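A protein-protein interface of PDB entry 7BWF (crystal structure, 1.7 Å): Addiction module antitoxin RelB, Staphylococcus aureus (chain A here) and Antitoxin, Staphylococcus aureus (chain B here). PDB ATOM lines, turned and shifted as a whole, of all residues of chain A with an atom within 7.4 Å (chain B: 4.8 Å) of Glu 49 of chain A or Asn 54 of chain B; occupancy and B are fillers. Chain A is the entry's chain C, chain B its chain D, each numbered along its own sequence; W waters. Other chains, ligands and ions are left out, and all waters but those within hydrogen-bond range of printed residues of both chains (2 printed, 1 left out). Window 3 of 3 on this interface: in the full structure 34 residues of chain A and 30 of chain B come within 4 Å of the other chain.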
ATOM      1  N   ALA A  41      -8.499   8.371 -16.936  1.00  0.00           N
ATOM      2  CA  ALA A  41      -8.638   8.486 -18.382  1.00  0.00           C
ATOM      3  C   ALA A  41      -9.745   9.460 -18.784  1.00  0.00           C
ATOM      4  O   ALA A  41      -9.708  10.022 -19.888  1.00  0.00           O
ATOM      5  CB  ALA A  41      -8.903   7.103 -18.981  1.00  0.00           C
ATOM      6  N   LEU A  42     -10.729   9.688 -17.913  1.00  0.00           N
ATOM      7  CA  LEU A  42     -11.928  10.432 -18.286  1.00  0.00           C
ATOM      8  C   LEU A  42     -12.058  11.774 -17.575  1.00  0.00           C
ATOM      9  O   LEU A  42     -13.096  12.434 -17.706  1.00  0.00           O
ATOM     10  CB  LEU A  42     -13.176   9.586 -18.010  1.00  0.00           C
ATOM     11  CG  LEU A  42     -13.501   8.521 -19.061  1.00  0.00           C
ATOM     12  CD1 LEU A  42     -14.749   7.716 -18.702  1.00  0.00           C
ATOM     13  CD2 LEU A  42     -13.659   9.151 -20.448  1.00  0.00           C
ATOM     14  N   GLY A  46      -8.555  18.758 -21.888  1.00  0.00           N
ATOM     15  CA  GLY A  46      -8.572  18.182 -23.216  1.00  0.00           C
ATOM     16  C   GLY A  46      -9.885  17.560 -23.638  1.00  0.00           C
ATOM     17  O   GLY A  46      -9.952  16.970 -24.728  1.00  0.00           O
ATOM     18  N   LYS A  47     -10.935  17.682 -22.813  1.00  0.00           N
ATOM     19  CA  LYS A  47     -12.262  17.178 -23.126  1.00  0.00           C
ATOM     20  C   LYS A  47     -12.176  15.687 -23.392  1.00  0.00           C
ATOM     21  O   LYS A  47     -12.378  15.259 -24.541  1.00  0.00           O
ATOM     22  CB  LYS A  47     -12.845  17.848 -24.359  1.00  0.00           C
ATOM     23  CG  LYS A  47     -12.931  19.342 -24.233  1.00  0.00           C
ATOM     24  CD  LYS A  47     -13.655  19.963 -25.403  1.00  0.00           C
ATOM     25  CE  LYS A  47     -14.421  21.239 -25.021  1.00  0.00           C
ATOM     26  NZ  LYS A  47     -13.549  22.439 -24.829  1.00  0.00           N
ATOM     27  N   PRO A  48     -11.836  14.878 -22.392  1.00  0.00           N
ATOM     28  CA  PRO A  48     -11.735  13.429 -22.617  1.00  0.00           C
ATOM     29  C   PRO A  48     -13.070  12.817 -22.997  1.00  0.00           C
ATOM     30  O   PRO A  48     -14.108  13.155 -22.427  1.00  0.00           O
ATOM     31  CB  PRO A  48     -11.241  12.888 -21.271  1.00  0.00           C
ATOM     32  CG  PRO A  48     -11.620  13.954 -20.287  1.00  0.00           C
ATOM     33  CD  PRO A  48     -11.479  15.244 -21.011  1.00  0.00           C
ATOM     34  N   GLU A  49     -13.032  11.941 -24.004  1.00  0.00           N
ATOM     35  CA  GLU A  49     -14.202  11.211 -24.458  1.00  0.00           C
ATOM     36  C   GLU A  49     -13.856   9.751 -24.726  1.00  0.00           C
ATOM     37  O   GLU A  49     -12.776   9.439 -25.235  1.00  0.00           O
ATOM     38  CB  GLU A  49     -14.760  11.832 -25.742  1.00  0.00           C
ATOM     39  CG  GLU A  49     -15.096  13.328 -25.647  1.00  0.00           C
ATOM     40  CD  GLU A  49     -16.339  13.606 -24.815  1.00  0.00           C
ATOM     41  OE1 GLU A  49     -17.012  12.631 -24.428  1.00  0.00           O
ATOM     42  OE2 GLU A  49     -16.648  14.791 -24.557  1.00  0.00           O
ATOM     43  N   LYS A  50     -14.788   8.866 -24.388  1.00  0.00           N
ATOM     44  CA  LYS A  50     -14.692   7.471 -24.793  1.00  0.00           C
ATOM     45  C   LYS A  50     -14.978   7.345 -26.287  1.00  0.00           C
ATOM     46  O   LYS A  50     -15.895   7.983 -26.813  1.00  0.00           O
ATOM     47  CB  LYS A  50     -15.697   6.614 -24.015  1.00  0.00           C
ATOM     48  CG  LYS A  50     -15.654   6.688 -22.502  1.00  0.00           C
ATOM     49  CD  LYS A  50     -16.702   5.717 -21.937  1.00  0.00           C
ATOM     50  CE  LYS A  50     -16.178   4.285 -21.882  1.00  0.00           C
ATOM     51  NZ  LYS A  50     -16.707   3.573 -20.682  1.00  0.00           N
ATOM     52  N   LEU A  51     -14.209   6.498 -26.966  1.00  0.00           N
ATOM     53  CA  LEU A  51     -14.414   6.224 -28.380  1.00  0.00           C
ATOM     54  C   LEU A  51     -15.207   4.934 -28.555  1.00  0.00           C
ATOM     55  O   LEU A  51     -15.218   4.057 -27.688  1.00  0.00           O
ATOM     56  CB  LEU A  51     -13.079   6.128 -29.130  1.00  0.00           C
ATOM     57  CG  LEU A  51     -12.250   7.406 -28.980  1.00  0.00           C
ATOM     58  CD1 LEU A  51     -10.882   7.276 -29.660  1.00  0.00           C
ATOM     59  CD2 LEU A  51     -12.989   8.651 -29.503  1.00  0.00           C
ATOM     60  N   LYS A  52     -15.873   4.837 -29.699  1.00  0.00           N
ATOM     61  CA  LYS A  52     -16.772   3.735 -30.021  1.00  0.00           C
ATOM     62  C   LYS A  52     -16.292   3.063 -31.308  1.00  0.00           C
ATOM     63  O   LYS A  52     -15.200   3.343 -31.810  1.00  0.00           O
ATOM     64  CB  LYS A  52     -18.218   4.255 -30.107  1.00  0.00           C
ATOM     65  CG  LYS A  52     -18.798   4.660 -28.735  1.00  0.00           C
ATOM     66  CD  LYS A  52     -20.223   5.237 -28.785  1.00  0.00           C
ATOM     67  CE  LYS A  52     -20.851   5.291 -27.373  1.00  0.00           C
ATOM     68  NZ  LYS A  52     -19.855   5.379 -26.260  1.00  0.00           N
ATOM     69  N   TYR A  58     -10.569   2.881 -26.218  1.00  0.00           N
ATOM     70  CA  TYR A  58      -9.663   4.013 -26.258  1.00  0.00           C
ATOM     71  C   TYR A  58     -10.406   5.312 -25.999  1.00  0.00           C
ATOM     72  O   TYR A  58     -11.636   5.368 -25.974  1.00  0.00           O
ATOM     73  CB  TYR A  58      -8.937   4.073 -27.599  1.00  0.00           C
ATOM     74  CG  TYR A  58      -7.827   3.060 -27.676  1.00  0.00           C
ATOM     75  CD1 TYR A  58      -8.108   1.709 -27.819  1.00  0.00           C
ATOM     76  CD2 TYR A  58      -6.498   3.448 -27.582  1.00  0.00           C
ATOM     77  CE1 TYR A  58      -7.097   0.776 -27.880  1.00  0.00           C
ATOM     78  CE2 TYR A  58      -5.482   2.521 -27.645  1.00  0.00           C
ATOM     79  CZ  TYR A  58      -5.787   1.187 -27.791  1.00  0.00           C
ATOM     80  OH  TYR A  58      -4.772   0.261 -27.852  1.00  0.00           O
ATOM     81  N   TYR A  59      -9.625   6.362 -25.779  1.00  0.00           N
ATOM     82  CA  TYR A  59     -10.155   7.669 -25.434  1.00  0.00           C
ATOM     83  C   TYR A  59      -9.519   8.720 -26.326  1.00  0.00           C
ATOM     84  O   TYR A  59      -8.434   8.521 -26.873  1.00  0.00           O
ATOM     85  CB  TYR A  59      -9.885   8.027 -23.957  1.00  0.00           C
ATOM     86  CG  TYR A  59     -10.392   6.992 -22.982  1.00  0.00           C
ATOM     87  CD1 TYR A  59      -9.590   5.934 -22.600  1.00  0.00           C
ATOM     88  CD2 TYR A  59     -11.661   7.084 -22.430  1.00  0.00           C
ATOM     89  CE1 TYR A  59     -10.041   4.979 -21.705  1.00  0.00           C
ATOM     90  CE2 TYR A  59     -12.121   6.133 -21.530  1.00  0.00           C
ATOM     91  CZ  TYR A  59     -11.309   5.084 -21.175  1.00  0.00           C
ATOM     92  OH  TYR A  59     -11.767   4.141 -20.280  1.00  0.00           O
ATOM     93  N   SER A  60     -10.192   9.858 -26.441  1.00  0.00           N
ATOM     94  CA  SER A  60      -9.639  11.003 -27.143  1.00  0.00           C
ATOM     95  C   SER A  60      -9.535  12.191 -26.201  1.00  0.00           C
ATOM     96  O   SER A  60     -10.422  12.436 -25.376  1.00  0.00           O
ATOM     97  CB  SER A  60     -10.488  11.401 -28.364  1.00  0.00           C
ATOM     98  OG  SER A  60     -11.621  12.163 -27.977  1.00  0.00           O
ATOM     99  N   ARG A  61      -8.445  12.927 -26.349  1.00  0.00           N
ATOM    100  CA  ARG A  61      -8.303  14.255 -25.782  1.00  0.00           C
ATOM    101  C   ARG A  61      -7.787  15.187 -26.867  1.00  0.00           C
ATOM    102  O   ARG A  61      -7.085  14.765 -27.789  1.00  0.00           O
ATOM    103  CB  ARG A  61      -7.353  14.259 -24.589  1.00  0.00           C
ATOM    104  CG  ARG A  61      -8.014  13.815 -23.290  1.00  0.00           C
ATOM    105  CD  ARG A  61      -7.081  13.978 -22.109  1.00  0.00           C
ATOM    106  NE  ARG A  61      -7.408  13.081 -21.003  1.00  0.00           N
ATOM    107  CZ  ARG A  61      -7.437  13.443 -19.720  1.00  0.00           C
ATOM    108  NH1 ARG A  61      -7.162  14.693 -19.358  1.00  0.00           N
ATOM    109  NH2 ARG A  61      -7.737  12.547 -18.788  1.00  0.00           N
ATOM    110  N   ARG A  62      -8.134  16.460 -26.749  1.00  0.00           N
ATOM    111  CA  ARG A  62      -7.807  17.426 -27.786  1.00  0.00           C
ATOM    112  C   ARG A  62      -6.425  18.016 -27.541  1.00  0.00           C
ATOM    113  O   ARG A  62      -6.190  18.664 -26.515  1.00  0.00           O
ATOM    114  CB  ARG A  62      -8.850  18.539 -27.829  1.00  0.00           C
ATOM    115  CG  ARG A  62     -10.216  18.116 -28.321  1.00  0.00           C
ATOM    116  CD  ARG A  62     -11.085  19.345 -28.559  1.00  0.00           C
ATOM    117  NE  ARG A  62     -12.494  19.008 -28.724  1.00  0.00           N
ATOM    118  CZ  ARG A  62     -13.290  19.553 -29.640  1.00  0.00           C
ATOM    119  NH1 ARG A  62     -12.823  20.469 -30.483  1.00  0.00           N
ATOM    120  NH2 ARG A  62     -14.561  19.181 -29.714  1.00  0.00           N
ATOM    121  N   LEU A  69      -5.061  13.301 -29.020  1.00  0.00           N
ATOM    122  CA  LEU A  69      -4.338  12.263 -28.297  1.00  0.00           C
ATOM    123  C   LEU A  69      -5.292  11.092 -28.102  1.00  0.00           C
ATOM    124  O   LEU A  69      -6.252  11.188 -27.332  1.00  0.00           O
ATOM    125  CB  LEU A  69      -3.827  12.792 -26.960  1.00  0.00           C
ATOM    126  CG  LEU A  69      -2.923  11.844 -26.173  1.00  0.00           C
ATOM    127  CD1 LEU A  69      -1.609  11.602 -26.916  1.00  0.00           C
ATOM    128  CD2 LEU A  69      -2.669  12.394 -24.771  1.00  0.00           C
ATOM    129  N   TYR A  71      -5.678   7.302 -26.829  1.00  0.00           N
ATOM    130  CA  TYR A  71      -4.936   6.580 -25.811  1.00  0.00           C
ATOM    131  C   TYR A  71      -5.855   5.639 -25.046  1.00  0.00           C
ATOM    132  O   TYR A  71      -7.082   5.681 -25.164  1.00  0.00           O
ATOM    133  CB  TYR A  71      -4.282   7.553 -24.824  1.00  0.00           C
ATOM    134  CG  TYR A  71      -5.318   8.342 -24.044  1.00  0.00           C
ATOM    135  CD1 TYR A  71      -5.855   9.516 -24.557  1.00  0.00           C
ATOM    136  CD2 TYR A  71      -5.786   7.898 -22.813  1.00  0.00           C
ATOM    137  CE1 TYR A  71      -6.812  10.233 -23.860  1.00  0.00           C
ATOM    138  CE2 TYR A  71      -6.743   8.615 -22.108  1.00  0.00           C
ATOM    139  CZ  TYR A  71      -7.250   9.782 -22.634  1.00  0.00           C
ATOM    140  OH  TYR A  71      -8.205  10.497 -21.943  1.00  0.00           O
ATOM    141  N   GLU B  50     -25.271  13.452 -23.467  1.00  0.00           N
ATOM    142  CA  GLU B  50     -24.309  14.346 -24.099  1.00  0.00           C
ATOM    143  C   GLU B  50     -22.979  13.630 -24.309  1.00  0.00           C
ATOM    144  O   GLU B  50     -22.302  13.840 -25.321  1.00  0.00           O
ATOM    145  CB  GLU B  50     -24.117  15.606 -23.249  1.00  0.00           C
ATOM    146  CG  GLU B  50     -23.131  16.597 -23.848  1.00  0.00           C
ATOM    147  CD  GLU B  50     -23.036  17.882 -23.035  1.00  0.00           C
ATOM    148  OE1 GLU B  50     -23.306  17.842 -21.818  1.00  0.00           O
ATOM    149  OE2 GLU B  50     -22.681  18.924 -23.610  1.00  0.00           O
ATOM    150  N   SER B  51     -22.596  12.766 -23.363  1.00  0.00           N
ATOM    151  CA  SER B  51     -21.341  12.032 -23.492  1.00  0.00           C
ATOM    152  C   SER B  51     -21.374  11.124 -24.716  1.00  0.00           C
ATOM    153  O   SER B  51     -20.439  11.119 -25.520  1.00  0.00           O
ATOM    154  CB  SER B  51     -21.063  11.216 -22.221  1.00  0.00           C
ATOM    155  OG  SER B  51     -20.727  12.057 -21.133  1.00  0.00           O
ATOM    156  N   ASP B  52     -22.453  10.356 -24.882  1.00  0.00           N
ATOM    157  CA  ASP B  52     -22.553   9.459 -26.032  1.00  0.00           C
ATOM    158  C   ASP B  52     -22.597  10.237 -27.340  1.00  0.00           C
ATOM    159  O   ASP B  52     -22.025   9.804 -28.344  1.00  0.00           O
ATOM    160  CB  ASP B  52     -23.784   8.564 -25.895  1.00  0.00           C
ATOM    161  CG  ASP B  52     -23.561   7.418 -24.918  1.00  0.00           C
ATOM    162  OD1 ASP B  52     -22.395   7.160 -24.545  1.00  0.00           O
ATOM    163  OD2 ASP B  52     -24.546   6.789 -24.503  1.00  0.00           O
ATOM    164  N   TYR B  53     -23.243  11.404 -27.344  1.00  0.00           N
ATOM    165  CA  TYR B  53     -23.200  12.245 -28.534  1.00  0.00           C
ATOM    166  C   TYR B  53     -21.767  12.658 -28.839  1.00  0.00           C
ATOM    167  O   TYR B  53     -21.293  12.508 -29.968  1.00  0.00           O
ATOM    168  CB  TYR B  53     -24.072  13.485 -28.358  1.00  0.00           C
ATOM    169  CG  TYR B  53     -23.888  14.489 -29.482  1.00  0.00           C
ATOM    170  CD1 TYR B  53     -24.556  14.335 -30.690  1.00  0.00           C
ATOM    171  CD2 TYR B  53     -23.040  15.581 -29.342  1.00  0.00           C
ATOM    172  CE1 TYR B  53     -24.395  15.245 -31.720  1.00  0.00           C
ATOM    173  CE2 TYR B  53     -22.872  16.497 -30.369  1.00  0.00           C
ATOM    174  CZ  TYR B  53     -23.555  16.325 -31.558  1.00  0.00           C
ATOM    175  OH  TYR B  53     -23.403  17.225 -32.594  1.00  0.00           O
ATOM    176  N   ASN B  54     -21.056  13.181 -27.837  1.00  0.00           N
ATOM    177  CA  ASN B  54     -19.676  13.602 -28.052  1.00  0.00           C
ATOM    178  C   ASN B  54     -18.812  12.426 -28.494  1.00  0.00           C
ATOM    179  O   ASN B  54     -17.928  12.584 -29.340  1.00  0.00           O
ATOM    180  CB  ASN B  54     -19.100  14.231 -26.780  1.00  0.00           C
ATOM    181  CG  ASN B  54     -19.665  15.606 -26.489  1.00  0.00           C
ATOM    182  OD1 ASN B  54     -20.179  16.282 -27.383  1.00  0.00           O
ATOM    183  ND2 ASN B  54     -19.601  16.015 -25.227  1.00  0.00           N
ATOM    184  N   SER B  55     -19.055  11.239 -27.932  1.00  0.00           N
ATOM    185  CA  SER B  55     -18.301  10.052 -28.332  1.00  0.00           C
ATOM    186  C   SER B  55     -18.534   9.731 -29.807  1.00  0.00           C
ATOM    187  O   SER B  55     -17.588   9.445 -30.550  1.00  0.00           O
ATOM    188  CB  SER B  55     -18.675   8.852 -27.442  1.00  0.00           C
ATOM    189  OG  SER B  55     -18.216   9.027 -26.110  1.00  0.00           O
ATOM    190  N   MET B  56     -19.789   9.800 -30.254  1.00  0.00           N
ATOM    191  CA  MET B  56     -20.112   9.473 -31.641  1.00  0.00           C
ATOM    192  C   MET B  56     -19.455  10.455 -32.604  1.00  0.00           C
ATOM    193  O   MET B  56     -18.878  10.053 -33.620  1.00  0.00           O
ATOM    194  CB  MET B  56     -21.633   9.454 -31.829  1.00  0.00           C
ATOM    195  CG  MET B  56     -22.187   8.042 -31.795  1.00  0.00           C
ATOM    196  SD  MET B  56     -23.887   7.865 -31.276  1.00  0.00           S
ATOM    197  CE  MET B  56     -24.665   9.085 -32.305  1.00  0.00           C
ATOM    198  N   MET B  57     -19.532  11.752 -32.298  1.00  0.00           N
ATOM    199  CA  MET B  57     -18.931  12.767 -33.159  1.00  0.00           C
ATOM    200  C   MET B  57     -17.410  12.650 -33.159  1.00  0.00           C
ATOM    201  O   MET B  57     -16.772  12.817 -34.203  1.00  0.00           O
ATOM    202  CB  MET B  57     -19.376  14.165 -32.711  1.00  0.00           C
ATOM    203  CG  MET B  57     -20.886  14.309 -32.561  1.00  0.00           C
ATOM    204  SD  MET B  57     -21.831  13.750 -34.000  1.00  0.00           S
ATOM    205  CE  MET B  57     -21.062  14.625 -35.351  1.00  0.00           C
ATOM    206  N   GLU B  58     -16.814  12.348 -32.000  1.00  0.00           N
ATOM    207  CA  GLU B  58     -15.368  12.137 -31.928  1.00  0.00           C
ATOM    208  C   GLU B  58     -14.953  10.910 -32.734  1.00  0.00           C
ATOM    209  O   GLU B  58     -13.969  10.952 -33.477  1.00  0.00           O
ATOM    210  CB  GLU B  58     -14.918  11.989 -30.467  1.00  0.00           C
ATOM    211  CG  GLU B  58     -14.494  13.281 -29.797  1.00  0.00           C
ATOM    212  CD  GLU B  58     -13.307  13.937 -30.492  1.00  0.00           C
ATOM    213  OE1 GLU B  58     -13.486  15.037 -31.032  1.00  0.00           O
ATOM    214  OE2 GLU B  58     -12.205  13.353 -30.509  1.00  0.00           O
HETATM  215  O   HOH W   1     -19.811   7.703 -23.981  1.00  0.00           O
HETATM  216  O   HOH W   2     -13.258  16.474 -28.330  1.00  0.00           O
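Hydrophobic or aromatic side chains of chain A that line the printed part of chain B: Leu 51.
Along chain B the printed residues that touch a printed residue of chain A span positions 51 to 58.
Among the printed residues, 7 pairs touch across the chains.
Water W2 bridges NE of Arg 62 of chain A (2.7 Å) and OE1 of Glu 58 of chain B (3.1 Å).
Water W1 lies within hydrogen-bond range of OD1 of Asp 52 of chain B (2.7 Å), OG of Ser 55 of chain B (3.0 Å) and NZ of Lys 52 of chain A (3.3 Å).
The side-chain amide nitrogen (ND2) of Asn 54 of chain B lies close to the backbone carbonyl oxygen (O) of Glu 50 of chain B, at 3.5 Å.
The backbone carbonyl oxygen of Ser 51 of chain B sits at hydrogen-bond distance from the side-chain hydroxyl of Ser 55 of chain B (3.1 Å).
N of Ser 60 of chain A sits at hydrogen-bond distance from O of Glu 49 of chain A, at 2.9 Å.
The backbone carbonyl oxygen of Tyr 58 of chain A is in hydrogen-bond range of the backbone NH of Leu 51 of chain A (3.0 Å).
Glu 49 of chain A touches Ser 51 of chain B.
CD2 of Leu 51 of chain A touches CB of Glu 58 of chain B, 3.97 Å away.
CB of Ser 55 of chain B touches NZ of Lys 52 of chain A (3.9 Å).
Printed residues of chain B within 4 Å of Glu 49 of chain A: Ser 51 (3.9 Å) and Asn 54 (3.3 Å).
Of chain A, only Glu 49 (3.3 Å) comes within 4 Å of Asn 54 of chain B.
Printed residues of chain B within 4 Å of Lys 50 of chain A: Ser 55 (2.6 Å).
Of the printed residues of chain A, Ser 51 of chain B touches Glu 49 (3.9 Å).
Arg 62 of chain A touches none of the printed residues of chain B.
The nearest printed residue of chain B that does not touch Lys 52 of chain A is Met 56 of chain B (4.6 Å).
The side-chain carboxylate (OE2) of Glu 49 of chain A sits at hydrogen-bond distance from the side-chain amide nitrogen (ND2) of Asn 54 of chain B (3.3 Å).
O of Lys 50 of chain A lies within hydrogen-bond range of OG of Ser 55 of chain B, at 2.6 Å.
The side-chain hydroxyl (OG) of Ser 60 of chain A lies within hydrogen-bond range of the side-chain carboxylate (OE2) of Glu 58 of chain B (2.9 Å).
OD1 of Asp 52 of chain B is in salt-bridge range of NZ of Lys 52 of chain A, 3.5 Å away.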
